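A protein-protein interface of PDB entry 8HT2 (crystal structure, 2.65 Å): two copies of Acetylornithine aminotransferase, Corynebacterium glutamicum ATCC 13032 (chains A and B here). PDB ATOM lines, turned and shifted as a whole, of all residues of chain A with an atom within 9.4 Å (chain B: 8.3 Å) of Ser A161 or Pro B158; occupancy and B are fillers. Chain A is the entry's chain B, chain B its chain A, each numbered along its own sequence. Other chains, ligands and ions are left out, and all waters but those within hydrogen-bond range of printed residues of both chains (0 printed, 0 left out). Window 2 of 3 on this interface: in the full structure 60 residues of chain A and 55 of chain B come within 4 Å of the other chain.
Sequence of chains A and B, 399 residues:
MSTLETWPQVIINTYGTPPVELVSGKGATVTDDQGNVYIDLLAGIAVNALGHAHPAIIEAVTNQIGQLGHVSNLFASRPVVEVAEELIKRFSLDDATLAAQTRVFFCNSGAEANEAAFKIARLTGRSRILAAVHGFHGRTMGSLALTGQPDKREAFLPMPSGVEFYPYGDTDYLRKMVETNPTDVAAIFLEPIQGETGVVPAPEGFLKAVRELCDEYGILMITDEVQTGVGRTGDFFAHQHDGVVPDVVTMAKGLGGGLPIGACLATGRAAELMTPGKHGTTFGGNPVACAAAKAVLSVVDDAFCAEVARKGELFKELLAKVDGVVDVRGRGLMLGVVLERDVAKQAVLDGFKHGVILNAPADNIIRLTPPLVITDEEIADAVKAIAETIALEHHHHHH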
ATOM      1  N   GLU A 115       2.061 -13.030  17.364  1.00  0.00           N
ATOM      2  CA  GLU A 115       1.932 -12.932  18.834  1.00  0.00           C
ATOM      3  C   GLU A 115       2.014 -14.353  19.348  1.00  0.00           C
ATOM      4  O   GLU A 115       2.706 -14.574  20.328  1.00  0.00           O
ATOM      5  CB  GLU A 115       0.593 -12.297  19.177  1.00  0.00           C
ATOM      6  CG  GLU A 115       0.613 -10.796  19.059  1.00  0.00           C
ATOM      7  CD  GLU A 115       0.927 -10.123  20.375  1.00  0.00           C
ATOM      8  OE1 GLU A 115       1.334 -10.832  21.304  1.00  0.00           O
ATOM      9  OE2 GLU A 115       0.756  -8.903  20.466  1.00  0.00           O
ATOM     10  N   PHE A 118       5.564 -15.140  19.262  1.00  0.00           N
ATOM     11  CA  PHE A 118       6.238 -14.534  20.438  1.00  0.00           C
ATOM     12  C   PHE A 118       5.948 -15.389  21.674  1.00  0.00           C
ATOM     13  O   PHE A 118       6.848 -15.549  22.497  1.00  0.00           O
ATOM     14  CB  PHE A 118       5.779 -13.080  20.593  1.00  0.00           C
ATOM     15  CG  PHE A 118       6.505 -12.214  21.592  1.00  0.00           C
ATOM     16  CD1 PHE A 118       6.197 -12.261  22.941  1.00  0.00           C
ATOM     17  CD2 PHE A 118       7.456 -11.305  21.173  1.00  0.00           C
ATOM     18  CE1 PHE A 118       6.858 -11.450  23.848  1.00  0.00           C
ATOM     19  CE2 PHE A 118       8.113 -10.490  22.080  1.00  0.00           C
ATOM     20  CZ  PHE A 118       7.816 -10.567  23.417  1.00  0.00           C
ATOM     21  N   LYS A 119       4.743 -15.945  21.773  1.00  0.00           N
ATOM     22  CA  LYS A 119       4.340 -16.709  22.981  1.00  0.00           C
ATOM     23  C   LYS A 119       5.070 -18.045  23.048  1.00  0.00           C
ATOM     24  O   LYS A 119       5.395 -18.470  24.147  1.00  0.00           O
ATOM     25  CB  LYS A 119       2.833 -16.965  22.982  1.00  0.00           C
ATOM     26  CG  LYS A 119       1.931 -15.764  23.172  1.00  0.00           C
ATOM     27  CD  LYS A 119       0.507 -16.125  23.493  1.00  0.00           C
ATOM     28  CE  LYS A 119       0.202 -15.915  24.956  1.00  0.00           C
ATOM     29  NZ  LYS A 119      -1.242 -15.942  25.272  1.00  0.00           N
ATOM     30  N   ALA A 121       7.996 -18.531  21.961  1.00  0.00           N
ATOM     31  CA  ALA A 121       9.356 -18.144  22.377  1.00  0.00           C
ATOM     32  C   ALA A 121       9.385 -17.837  23.871  1.00  0.00           C
ATOM     33  O   ALA A 121      10.430 -18.010  24.474  1.00  0.00           O
ATOM     34  CB  ALA A 121       9.801 -16.972  21.565  1.00  0.00           C
ATOM     35  N   ARG A 122       8.267 -17.430  24.453  1.00  0.00           N
ATOM     36  CA  ARG A 122       8.238 -17.227  25.919  1.00  0.00           C
ATOM     37  C   ARG A 122       8.141 -18.588  26.596  1.00  0.00           C
ATOM     38  O   ARG A 122       8.681 -18.726  27.695  1.00  0.00           O
ATOM     39  CB  ARG A 122       7.059 -16.346  26.324  1.00  0.00           C
ATOM     40  CG  ARG A 122       7.066 -14.955  25.714  1.00  0.00           C
ATOM     41  CD  ARG A 122       7.221 -13.890  26.773  1.00  0.00           C
ATOM     42  NE  ARG A 122       8.612 -13.502  26.881  1.00  0.00           N
ATOM     43  CZ  ARG A 122       9.039 -12.260  27.019  1.00  0.00           C
ATOM     44  NH1 ARG A 122      10.335 -12.026  27.103  1.00  0.00           N
ATOM     45  NH2 ARG A 122       8.180 -11.261  27.089  1.00  0.00           N
ATOM     46  N   LEU A 123       7.533 -19.564  25.933  1.00  0.00           N
ATOM     47  CA  LEU A 123       7.310 -20.900  26.531  1.00  0.00           C
ATOM     48  C   LEU A 123       8.592 -21.731  26.518  1.00  0.00           C
ATOM     49  O   LEU A 123       8.573 -22.822  27.086  1.00  0.00           O
ATOM     50  CB  LEU A 123       6.207 -21.582  25.724  1.00  0.00           C
ATOM     51  CG  LEU A 123       4.782 -21.177  26.083  1.00  0.00           C
ATOM     52  CD1 LEU A 123       3.790 -21.786  25.110  1.00  0.00           C
ATOM     53  CD2 LEU A 123       4.450 -21.581  27.506  1.00  0.00           C
ATOM     54  N   GLY A 125      11.331 -20.707  27.930  1.00  0.00           N
ATOM     55  CA  GLY A 125      11.982 -20.415  29.216  1.00  0.00           C
ATOM     56  C   GLY A 125      13.110 -19.434  29.027  1.00  0.00           C
ATOM     57  O   GLY A 125      13.593 -18.901  30.023  1.00  0.00           O
ATOM     58  N   ARG A 126      13.496 -19.203  27.778  1.00  0.00           N
ATOM     59  CA  ARG A 126      14.603 -18.270  27.465  1.00  0.00           C
ATOM     60  C   ARG A 126      14.034 -16.860  27.304  1.00  0.00           C
ATOM     61  O   ARG A 126      12.849 -16.756  26.978  1.00  0.00           O
ATOM     62  CB  ARG A 126      15.435 -18.818  26.304  1.00  0.00           C
ATOM     63  CG  ARG A 126      15.837 -20.275  26.464  1.00  0.00           C
ATOM     64  CD  ARG A 126      16.186 -20.928  25.143  1.00  0.00           C
ATOM     65  NE  ARG A 126      16.939 -22.162  25.289  1.00  0.00           N
ATOM     66  CZ  ARG A 126      17.941 -22.530  24.503  1.00  0.00           C
ATOM     67  NH1 ARG A 126      18.328 -21.751  23.511  1.00  0.00           N
ATOM     68  NH2 ARG A 126      18.557 -23.676  24.717  1.00  0.00           N
ATOM     69  N   SER A 127      14.852 -15.828  27.505  1.00  0.00           N
ATOM     70  CA  SER A 127      14.351 -14.431  27.524  1.00  0.00           C
ATOM     71  C   SER A 127      14.632 -13.684  26.227  1.00  0.00           C
ATOM     72  O   SER A 127      13.785 -12.881  25.836  1.00  0.00           O
ATOM     73  CB  SER A 127      14.988 -13.709  28.659  1.00  0.00           C
ATOM     74  OG  SER A 127      16.342 -13.408  28.371  1.00  0.00           O
ATOM     75  N   ARG A 128      15.761 -13.955  25.595  1.00  0.00           N
ATOM     76  CA  ARG A 128      16.206 -13.219  24.377  1.00  0.00           C
ATOM     77  C   ARG A 128      15.464 -13.725  23.128  1.00  0.00           C
ATOM     78  O   ARG A 128      15.484 -14.960  22.868  1.00  0.00           O
ATOM     79  CB  ARG A 128      17.703 -13.403  24.124  1.00  0.00           C
ATOM     80  CG  ARG A 128      18.605 -13.010  25.286  1.00  0.00           C
ATOM     81  CD  ARG A 128      20.064 -13.245  24.978  1.00  0.00           C
ATOM     82  NE  ARG A 128      20.553 -12.326  23.967  1.00  0.00           N
ATOM     83  CZ  ARG A 128      21.615 -12.538  23.169  1.00  0.00           C
ATOM     84  NH1 ARG A 128      22.313 -13.665  23.253  1.00  0.00           N
ATOM     85  NH2 ARG A 128      21.977 -11.610  22.285  1.00  0.00           N
ATOM     86  N   ILE A 129      14.841 -12.799  22.386  1.00  0.00           N
ATOM     87  CA  ILE A 129      14.270 -12.980  21.018  1.00  0.00           C
ATOM     88  C   ILE A 129      14.985 -11.987  20.110  1.00  0.00           C
ATOM     89  O   ILE A 129      15.094 -10.816  20.512  1.00  0.00           O
ATOM     90  CB  ILE A 129      12.752 -12.719  21.002  1.00  0.00           C
ATOM     91  CG1 ILE A 129      12.050 -13.428  22.155  1.00  0.00           C
ATOM     92  CG2 ILE A 129      12.130 -13.079  19.658  1.00  0.00           C
ATOM     93  CD1 ILE A 129      10.563 -13.340  22.077  1.00  0.00           C
ATOM     94  N   LEU A 130      15.432 -12.432  18.935  1.00  0.00           N
ATOM     95  CA  LEU A 130      16.227 -11.609  17.989  1.00  0.00           C
ATOM     96  C   LEU A 130      15.462 -11.477  16.671  1.00  0.00           C
ATOM     97  O   LEU A 130      14.970 -12.504  16.160  1.00  0.00           O
ATOM     98  CB  LEU A 130      17.584 -12.285  17.799  1.00  0.00           C
ATOM     99  CG  LEU A 130      18.186 -12.805  19.099  1.00  0.00           C
ATOM    100  CD1 LEU A 130      19.353 -13.762  18.868  1.00  0.00           C
ATOM    101  CD2 LEU A 130      18.566 -11.629  19.973  1.00  0.00           C
ATOM    102  N   MET A 141       0.896  -5.323  20.658  1.00  0.00           N
ATOM    103  CA  MET A 141       2.070  -5.108  21.543  1.00  0.00           C
ATOM    104  C   MET A 141       3.218  -6.095  21.330  1.00  0.00           C
ATOM    105  O   MET A 141       4.347  -5.627  21.197  1.00  0.00           O
ATOM    106  CB  MET A 141       1.663  -5.058  23.017  1.00  0.00           C
ATOM    107  CG  MET A 141       1.004  -3.756  23.403  1.00  0.00           C
ATOM    108  SD  MET A 141       1.924  -2.315  22.826  1.00  0.00           S
ATOM    109  CE  MET A 141       3.235  -2.259  24.043  1.00  0.00           C
ATOM    110  N   GLY A 142       2.950  -7.398  21.331  1.00  0.00           N
ATOM    111  CA  GLY A 142       4.040  -8.378  21.209  1.00  0.00           C
ATOM    112  C   GLY A 142       4.606  -8.436  19.811  1.00  0.00           C
ATOM    113  O   GLY A 142       5.813  -8.611  19.676  1.00  0.00           O
ATOM    114  N   ALA A 145       6.733  -5.510  19.395  1.00  0.00           N
ATOM    115  CA  ALA A 145       7.995  -5.741  20.119  1.00  0.00           C
ATOM    116  C   ALA A 145       9.034  -6.348  19.167  1.00  0.00           C
ATOM    117  O   ALA A 145      10.237  -6.176  19.451  1.00  0.00           O
ATOM    118  CB  ALA A 145       7.745  -6.599  21.332  1.00  0.00           C
ATOM    119  N   LEU A 146       8.575  -7.009  18.093  1.00  0.00           N
ATOM    120  CA  LEU A 146       9.410  -7.765  17.127  1.00  0.00           C
ATOM    121  C   LEU A 146       9.761  -6.875  15.926  1.00  0.00           C
ATOM    122  O   LEU A 146      10.724  -7.217  15.180  1.00  0.00           O
ATOM    123  CB  LEU A 146       8.627  -9.003  16.675  1.00  0.00           C
ATOM    124  CG  LEU A 146       8.316 -10.041  17.758  1.00  0.00           C
ATOM    125  CD1 LEU A 146       7.303 -11.070  17.265  1.00  0.00           C
ATOM    126  CD2 LEU A 146       9.588 -10.735  18.204  1.00  0.00           C
ATOM    127  N   PRO A 158       6.579   1.219  27.724  1.00  0.00           N
ATOM    128  CA  PRO A 158       7.263  -0.063  27.505  1.00  0.00           C
ATOM    129  C   PRO A 158       6.734  -1.129  26.531  1.00  0.00           C
ATOM    130  O   PRO A 158       5.570  -1.243  26.346  1.00  0.00           O
ATOM    131  CB  PRO A 158       7.218  -0.680  28.909  1.00  0.00           C
ATOM    132  CG  PRO A 158       7.156   0.492  29.832  1.00  0.00           C
ATOM    133  CD  PRO A 158       6.208   1.424  29.120  1.00  0.00           C
ATOM    134  N   MET A 159       7.638  -1.877  25.906  1.00  0.00           N
ATOM    135  CA  MET A 159       7.226  -3.018  25.052  1.00  0.00           C
ATOM    136  C   MET A 159       7.385  -4.272  25.912  1.00  0.00           C
ATOM    137  O   MET A 159       8.059  -4.145  26.938  1.00  0.00           O
ATOM    138  CB  MET A 159       8.142  -3.150  23.836  1.00  0.00           C
ATOM    139  CG  MET A 159       8.384  -1.850  23.112  1.00  0.00           C
ATOM    140  SD  MET A 159       6.893  -1.223  22.317  1.00  0.00           S
ATOM    141  CE  MET A 159       6.346  -2.698  21.472  1.00  0.00           C
ATOM    142  N   PRO A 160       6.802  -5.466  25.626  1.00  0.00           N
ATOM    143  CA  PRO A 160       7.100  -6.645  26.436  1.00  0.00           C
ATOM    144  C   PRO A 160       8.602  -6.862  26.179  1.00  0.00           C
ATOM    145  O   PRO A 160       9.018  -6.751  25.051  1.00  0.00           O
ATOM    146  CB  PRO A 160       6.230  -7.781  25.884  1.00  0.00           C
ATOM    147  CG  PRO A 160       5.776  -7.312  24.537  1.00  0.00           C
ATOM    148  CD  PRO A 160       5.693  -5.813  24.690  1.00  0.00           C
ATOM    149  N   SER A 161       9.381  -7.211  27.200  1.00  0.00           N
ATOM    150  CA  SER A 161      10.862  -7.262  27.079  1.00  0.00           C
ATOM    151  C   SER A 161      11.421  -8.514  26.405  1.00  0.00           C
ATOM    152  O   SER A 161      10.690  -9.501  26.316  1.00  0.00           O
ATOM    153  CB  SER A 161      11.452  -7.106  28.433  1.00  0.00           C
ATOM    154  OG  SER A 161      11.841  -8.364  28.955  1.00  0.00           O
ATOM    155  N   GLY A 162      12.668  -8.444  25.918  1.00  0.00           N
ATOM    156  CA  GLY A 162      13.340  -9.635  25.362  1.00  0.00           C
ATOM    157  C   GLY A 162      13.877  -9.471  23.958  1.00  0.00           C
ATOM    158  O   GLY A 162      14.821 -10.175  23.623  1.00  0.00           O
ATOM    159  N   VAL A 163      13.323  -8.550  23.182  1.00  0.00           N
ATOM    160  CA  VAL A 163      13.711  -8.425  21.747  1.00  0.00           C
ATOM    161  C   VAL A 163      14.988  -7.591  21.619  1.00  0.00           C
ATOM    162  O   VAL A 163      15.048  -6.558  22.263  1.00  0.00           O
ATOM    163  CB  VAL A 163      12.579  -7.829  20.899  1.00  0.00           C
ATOM    164  CG1 VAL A 163      12.963  -7.830  19.430  1.00  0.00           C
ATOM    165  CG2 VAL A 163      11.255  -8.557  21.134  1.00  0.00           C
ATOM    166  N   GLU A 164      15.953  -8.063  20.817  1.00  0.00           N
ATOM    167  CA  GLU A 164      17.138  -7.323  20.282  1.00  0.00           C
ATOM    168  C   GLU A 164      17.156  -7.463  18.750  1.00  0.00           C
ATOM    169  O   GLU A 164      16.551  -8.413  18.234  1.00  0.00           O
ATOM    170  CB  GLU A 164      18.457  -7.881  20.813  1.00  0.00           C
ATOM    171  CG  GLU A 164      18.550  -7.942  22.324  1.00  0.00           C
ATOM    172  CD  GLU A 164      19.467  -9.056  22.820  1.00  0.00           C
ATOM    173  OE1 GLU A 164      20.687  -8.946  22.569  1.00  0.00           O
ATOM    174  OE2 GLU A 164      18.966 -10.050  23.434  1.00  0.00           O
ATOM    175  N   ASP A 184      20.305 -18.382  26.321  1.00  0.00           N
ATOM    176  CA  ASP A 184      19.187 -17.471  26.696  1.00  0.00           C
ATOM    177  C   ASP A 184      18.495 -16.942  25.425  1.00  0.00           C
ATOM    178  O   ASP A 184      17.641 -16.050  25.561  1.00  0.00           O
ATOM    179  CB  ASP A 184      19.666 -16.350  27.626  1.00  0.00           C
ATOM    180  CG  ASP A 184      18.685 -15.976  28.731  1.00  0.00           C
ATOM    181  OD1 ASP A 184      17.471 -16.011  28.484  1.00  0.00           O
ATOM    182  OD2 ASP A 184      19.152 -15.666  29.844  1.00  0.00           O
ATOM    183  N   ALA A 186      15.745 -17.750  22.861  1.00  0.00           N
ATOM    184  CA  ALA A 186      14.483 -18.499  22.701  1.00  0.00           C
ATOM    185  C   ALA A 186      14.221 -18.773  21.225  1.00  0.00           C
ATOM    186  O   ALA A 186      13.919 -19.912  20.884  1.00  0.00           O
ATOM    187  CB  ALA A 186      13.368 -17.687  23.280  1.00  0.00           C
ATOM    188  N   MET B 141      -0.274 -10.396  23.746  1.00  0.00           N
ATOM    189  CA  MET B 141       0.575  -9.819  24.826  1.00  0.00           C
ATOM    190  C   MET B 141      -0.092  -8.666  25.579  1.00  0.00           C
ATOM    191  O   MET B 141      -0.193  -8.773  26.802  1.00  0.00           O
ATOM    192  CB  MET B 141       1.941  -9.375  24.303  1.00  0.00           C
ATOM    193  CG  MET B 141       2.976 -10.476  24.290  1.00  0.00           C
ATOM    194  SD  MET B 141       3.152 -11.339  25.864  1.00  0.00           S
ATOM    195  CE  MET B 141       2.583 -12.968  25.396  1.00  0.00           C
ATOM    196  N   LEU B 144      -3.455  -9.564  27.008  1.00  0.00           N
ATOM    197  CA  LEU B 144      -3.264 -10.534  28.127  1.00  0.00           C
ATOM    198  C   LEU B 144      -2.757  -9.792  29.374  1.00  0.00           C
ATOM    199  O   LEU B 144      -3.145 -10.155  30.502  1.00  0.00           O
ATOM    200  CB  LEU B 144      -2.291 -11.626  27.670  1.00  0.00           C
ATOM    201  CG  LEU B 144      -2.003 -12.746  28.668  1.00  0.00           C
ATOM    202  CD1 LEU B 144      -3.289 -13.364  29.193  1.00  0.00           C
ATOM    203  CD2 LEU B 144      -1.127 -13.815  28.037  1.00  0.00           C
ATOM    204  N   ALA B 145      -1.956  -8.740  29.178  1.00  0.00           N
ATOM    205  CA  ALA B 145      -1.451  -7.865  30.258  1.00  0.00           C
ATOM    206  C   ALA B 145      -2.624  -7.248  31.032  1.00  0.00           C
ATOM    207  O   ALA B 145      -2.400  -6.924  32.240  1.00  0.00           O
ATOM    208  CB  ALA B 145      -0.521  -6.808  29.708  1.00  0.00           C
ATOM    209  N   ARG B 153      -1.304 -15.719  32.440  1.00  0.00           N
ATOM    210  CA  ARG B 153      -0.132 -14.829  32.164  1.00  0.00           C
ATOM    211  C   ARG B 153       1.187 -15.520  32.539  1.00  0.00           C
ATOM    212  O   ARG B 153       2.163 -15.359  31.779  1.00  0.00           O
ATOM    213  CB  ARG B 153      -0.253 -13.496  32.915  1.00  0.00           C
ATOM    214  CG  ARG B 153      -1.571 -12.761  32.711  1.00  0.00           C
ATOM    215  CD  ARG B 153      -1.534 -11.357  33.302  1.00  0.00           C
ATOM    216  NE  ARG B 153      -1.168 -11.319  34.717  1.00  0.00           N
ATOM    217  CZ  ARG B 153      -2.004 -11.075  35.732  1.00  0.00           C
ATOM    218  NH1 ARG B 153      -3.288 -10.826  35.536  1.00  0.00           N
ATOM    219  NH2 ARG B 153      -1.547 -11.059  36.966  1.00  0.00           N
ATOM    220  N   GLU B 154       1.223 -16.215  33.671  1.00  0.00           N
ATOM    221  CA  GLU B 154       2.482 -16.801  34.207  1.00  0.00           C
ATOM    222  C   GLU B 154       3.394 -17.370  33.125  1.00  0.00           C
ATOM    223  O   GLU B 154       4.599 -17.097  33.182  1.00  0.00           O
ATOM    224  CB  GLU B 154       2.156 -17.849  35.270  1.00  0.00           C
ATOM    225  CG  GLU B 154       1.970 -17.264  36.654  1.00  0.00           C
ATOM    226  CD  GLU B 154       3.225 -16.660  37.257  1.00  0.00           C
ATOM    227  OE1 GLU B 154       4.314 -17.220  37.042  1.00  0.00           O
ATOM    228  OE2 GLU B 154       3.107 -15.634  37.946  1.00  0.00           O
ATOM    229  N   ALA B 155       2.848 -18.118  32.176  1.00  0.00           N
ATOM    230  CA  ALA B 155       3.681 -18.803  31.167  1.00  0.00           C
ATOM    231  C   ALA B 155       4.357 -17.842  30.193  1.00  0.00           C
ATOM    232  O   ALA B 155       5.245 -18.299  29.469  1.00  0.00           O
ATOM    233  CB  ALA B 155       2.795 -19.751  30.431  1.00  0.00           C
ATOM    234  N   PHE B 156       3.965 -16.570  30.167  1.00  0.00           N
ATOM    235  CA  PHE B 156       4.493 -15.651  29.131  1.00  0.00           C
ATOM    236  C   PHE B 156       4.988 -14.350  29.755  1.00  0.00           C
ATOM    237  O   PHE B 156       4.957 -13.319  29.092  1.00  0.00           O
ATOM    238  CB  PHE B 156       3.430 -15.423  28.055  1.00  0.00           C
ATOM    239  CG  PHE B 156       2.546 -16.603  27.752  1.00  0.00           C
ATOM    240  CD1 PHE B 156       2.949 -17.574  26.853  1.00  0.00           C
ATOM    241  CD2 PHE B 156       1.312 -16.743  28.365  1.00  0.00           C
ATOM    242  CE1 PHE B 156       2.136 -18.658  26.575  1.00  0.00           C
ATOM    243  CE2 PHE B 156       0.505 -17.833  28.090  1.00  0.00           C
ATOM    244  CZ  PHE B 156       0.918 -18.787  27.194  1.00  0.00           C
ATOM    245  N   LEU B 157       5.430 -14.415  31.002  1.00  0.00           N
ATOM    246  CA  LEU B 157       6.014 -13.239  31.681  1.00  0.00           C
ATOM    247  C   LEU B 157       7.447 -13.106  31.158  1.00  0.00           C
ATOM    248  O   LEU B 157       8.057 -14.151  30.898  1.00  0.00           O
ATOM    249  CB  LEU B 157       6.014 -13.547  33.180  1.00  0.00           C
ATOM    250  CG  LEU B 157       5.016 -12.809  34.066  1.00  0.00           C
ATOM    251  CD1 LEU B 157       3.613 -12.900  33.510  1.00  0.00           C
ATOM    252  CD2 LEU B 157       5.047 -13.384  35.471  1.00  0.00           C
ATOM    253  N   PRO B 158       8.037 -11.907  30.980  1.00  0.00           N
ATOM    254  CA  PRO B 158       7.398 -10.635  31.309  1.00  0.00           C
ATOM    255  C   PRO B 158       6.260 -10.134  30.408  1.00  0.00           C
ATOM    256  O   PRO B 158       6.274 -10.407  29.240  1.00  0.00           O
ATOM    257  CB  PRO B 158       8.556  -9.634  31.226  1.00  0.00           C
ATOM    258  CG  PRO B 158       9.801 -10.471  31.267  1.00  0.00           C
ATOM    259  CD  PRO B 158       9.408 -11.725  30.528  1.00  0.00           C
ATOM    260  N   MET B 159       5.317  -9.402  30.986  1.00  0.00           N
ATOM    261  CA  MET B 159       4.198  -8.811  30.217  1.00  0.00           C
ATOM    262  C   MET B 159       4.507  -7.356  29.903  1.00  0.00           C
ATOM    263  O   MET B 159       5.474  -6.829  30.453  1.00  0.00           O
ATOM    264  CB  MET B 159       2.935  -8.808  31.079  1.00  0.00           C
ATOM    265  CG  MET B 159       2.401 -10.174  31.400  1.00  0.00           C
ATOM    266  SD  MET B 159       1.160 -10.696  30.218  1.00  0.00           S
ATOM    267  CE  MET B 159       1.853 -12.271  29.733  1.00  0.00           C
ATOM    268  N   PRO B 160       3.773  -6.707  28.981  1.00  0.00           N
ATOM    269  CA  PRO B 160       3.916  -5.271  28.782  1.00  0.00           C
ATOM    270  C   PRO B 160       3.585  -4.626  30.134  1.00  0.00           C
ATOM    271  O   PRO B 160       2.529  -4.871  30.652  1.00  0.00           O
ATOM    272  CB  PRO B 160       2.843  -4.961  27.738  1.00  0.00           C
ATOM    273  CG  PRO B 160       2.647  -6.242  26.983  1.00  0.00           C
ATOM    274  CD  PRO B 160       2.871  -7.328  28.007  1.00  0.00           C
ATOM    275  N   SER B 161       4.480  -3.806  30.665  1.00  0.00           N
ATOM    276  CA  SER B 161       4.290  -3.244  32.027  1.00  0.00           C
ATOM    277  C   SER B 161       3.211  -2.157  32.085  1.00  0.00           C
ATOM    278  O   SER B 161       2.929  -1.559  31.048  1.00  0.00           O
ATOM    279  CB  SER B 161       5.602  -2.740  32.550  1.00  0.00           C
ATOM    280  OG  SER B 161       5.704  -1.338  32.396  1.00  0.00           O
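NH2 of Arg A122 is in hydrogen-bond range of O of Pro B158, at 3.0 Å.
N of Met B141 lies within hydrogen-bond range of OE1 of Glu A115, at 3.0 Å.
OE2 of Glu A115 sits at hydrogen-bond distance from N of Gly A142 (2.8 Å).
NH1 of Arg A122 lies within hydrogen-bond range of O of Ser A161 (2.7 Å).
CD1 of Phe A118 touches CG of Met B141 (3.9 Å).
Lys A119 touches Met B141.
Lys A119 touches Leu B144 (NZ to CD2, 3.5 Å).
Lys A119 touches Phe B156.
Arg A122 touches Ala B155 (O to O, 3.9 Å).
Phe B156 touches Arg A122 (O to CD, 3.3 Å).
Leu A123 touches Ala B155 (CD2 to CB, 3.8 Å).
Phe B156 touches Leu A123.
CB of Met B141 touches N of Gly A142 (3.7 Å).
CD of Pro A160 touches CG of Pro B160 (3.8 Å).
Of the printed residues of chain B, Ser A161 touches Pro B158.
Of the printed residues of chain B, Pro A160 touches Pro B160.
Of the printed residues of chain A, Phe B156 touches Lys A119 (3.7 Å), Arg A122 (3.3 Å) and Leu A123 (3.7 Å).
Ser A127 touches none of the printed residues of chain B.
The nearest residue of chain B that does not touch Ser A161 is Met B159 (5.1 Å).
The nearest residue of chain A that does not touch Pro B158 is Pro A160 (4.3 Å).
The nearest printed residue of chain B that does not touch Arg A122 is Leu B157 (4.1 Å).
Of the 25 printed residues of chain A, 9 touch a printed residue of chain B.
Printed residues of chain A that touch a printed residue of chain B: Glu A115, Phe A118, Lys A119, Arg A122, Leu A123, Gly A142, Pro A158, Pro A160 and Ser A161.
Hydrophobic or aromatic side chains of chain A that line the printed part of chain B: Phe A118, Leu A123, Pro A158 and Pro A160.
Along chain A the printed residues that touch a printed residue of chain B span positions 115 to 161.
Hydrophobic or aromatic side chains of chain B within 4 Å of the printed part of chain A: Met B141, Leu B144, Ala B155, Phe B156, Pro B158 and Pro B160.
Among the printed residues, 14 pairs touch across the chains.
Pro A158 touches Ser B161, and with the chains exchanged Ser A161 touches Pro B158.
Pro A160 touches its own counterpart, Pro B160.
6 positions are printed for both chains.
Of the 14 pairs that touch across the chains among the printed residues, 3 have their exchanged pair printed and touching as well.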
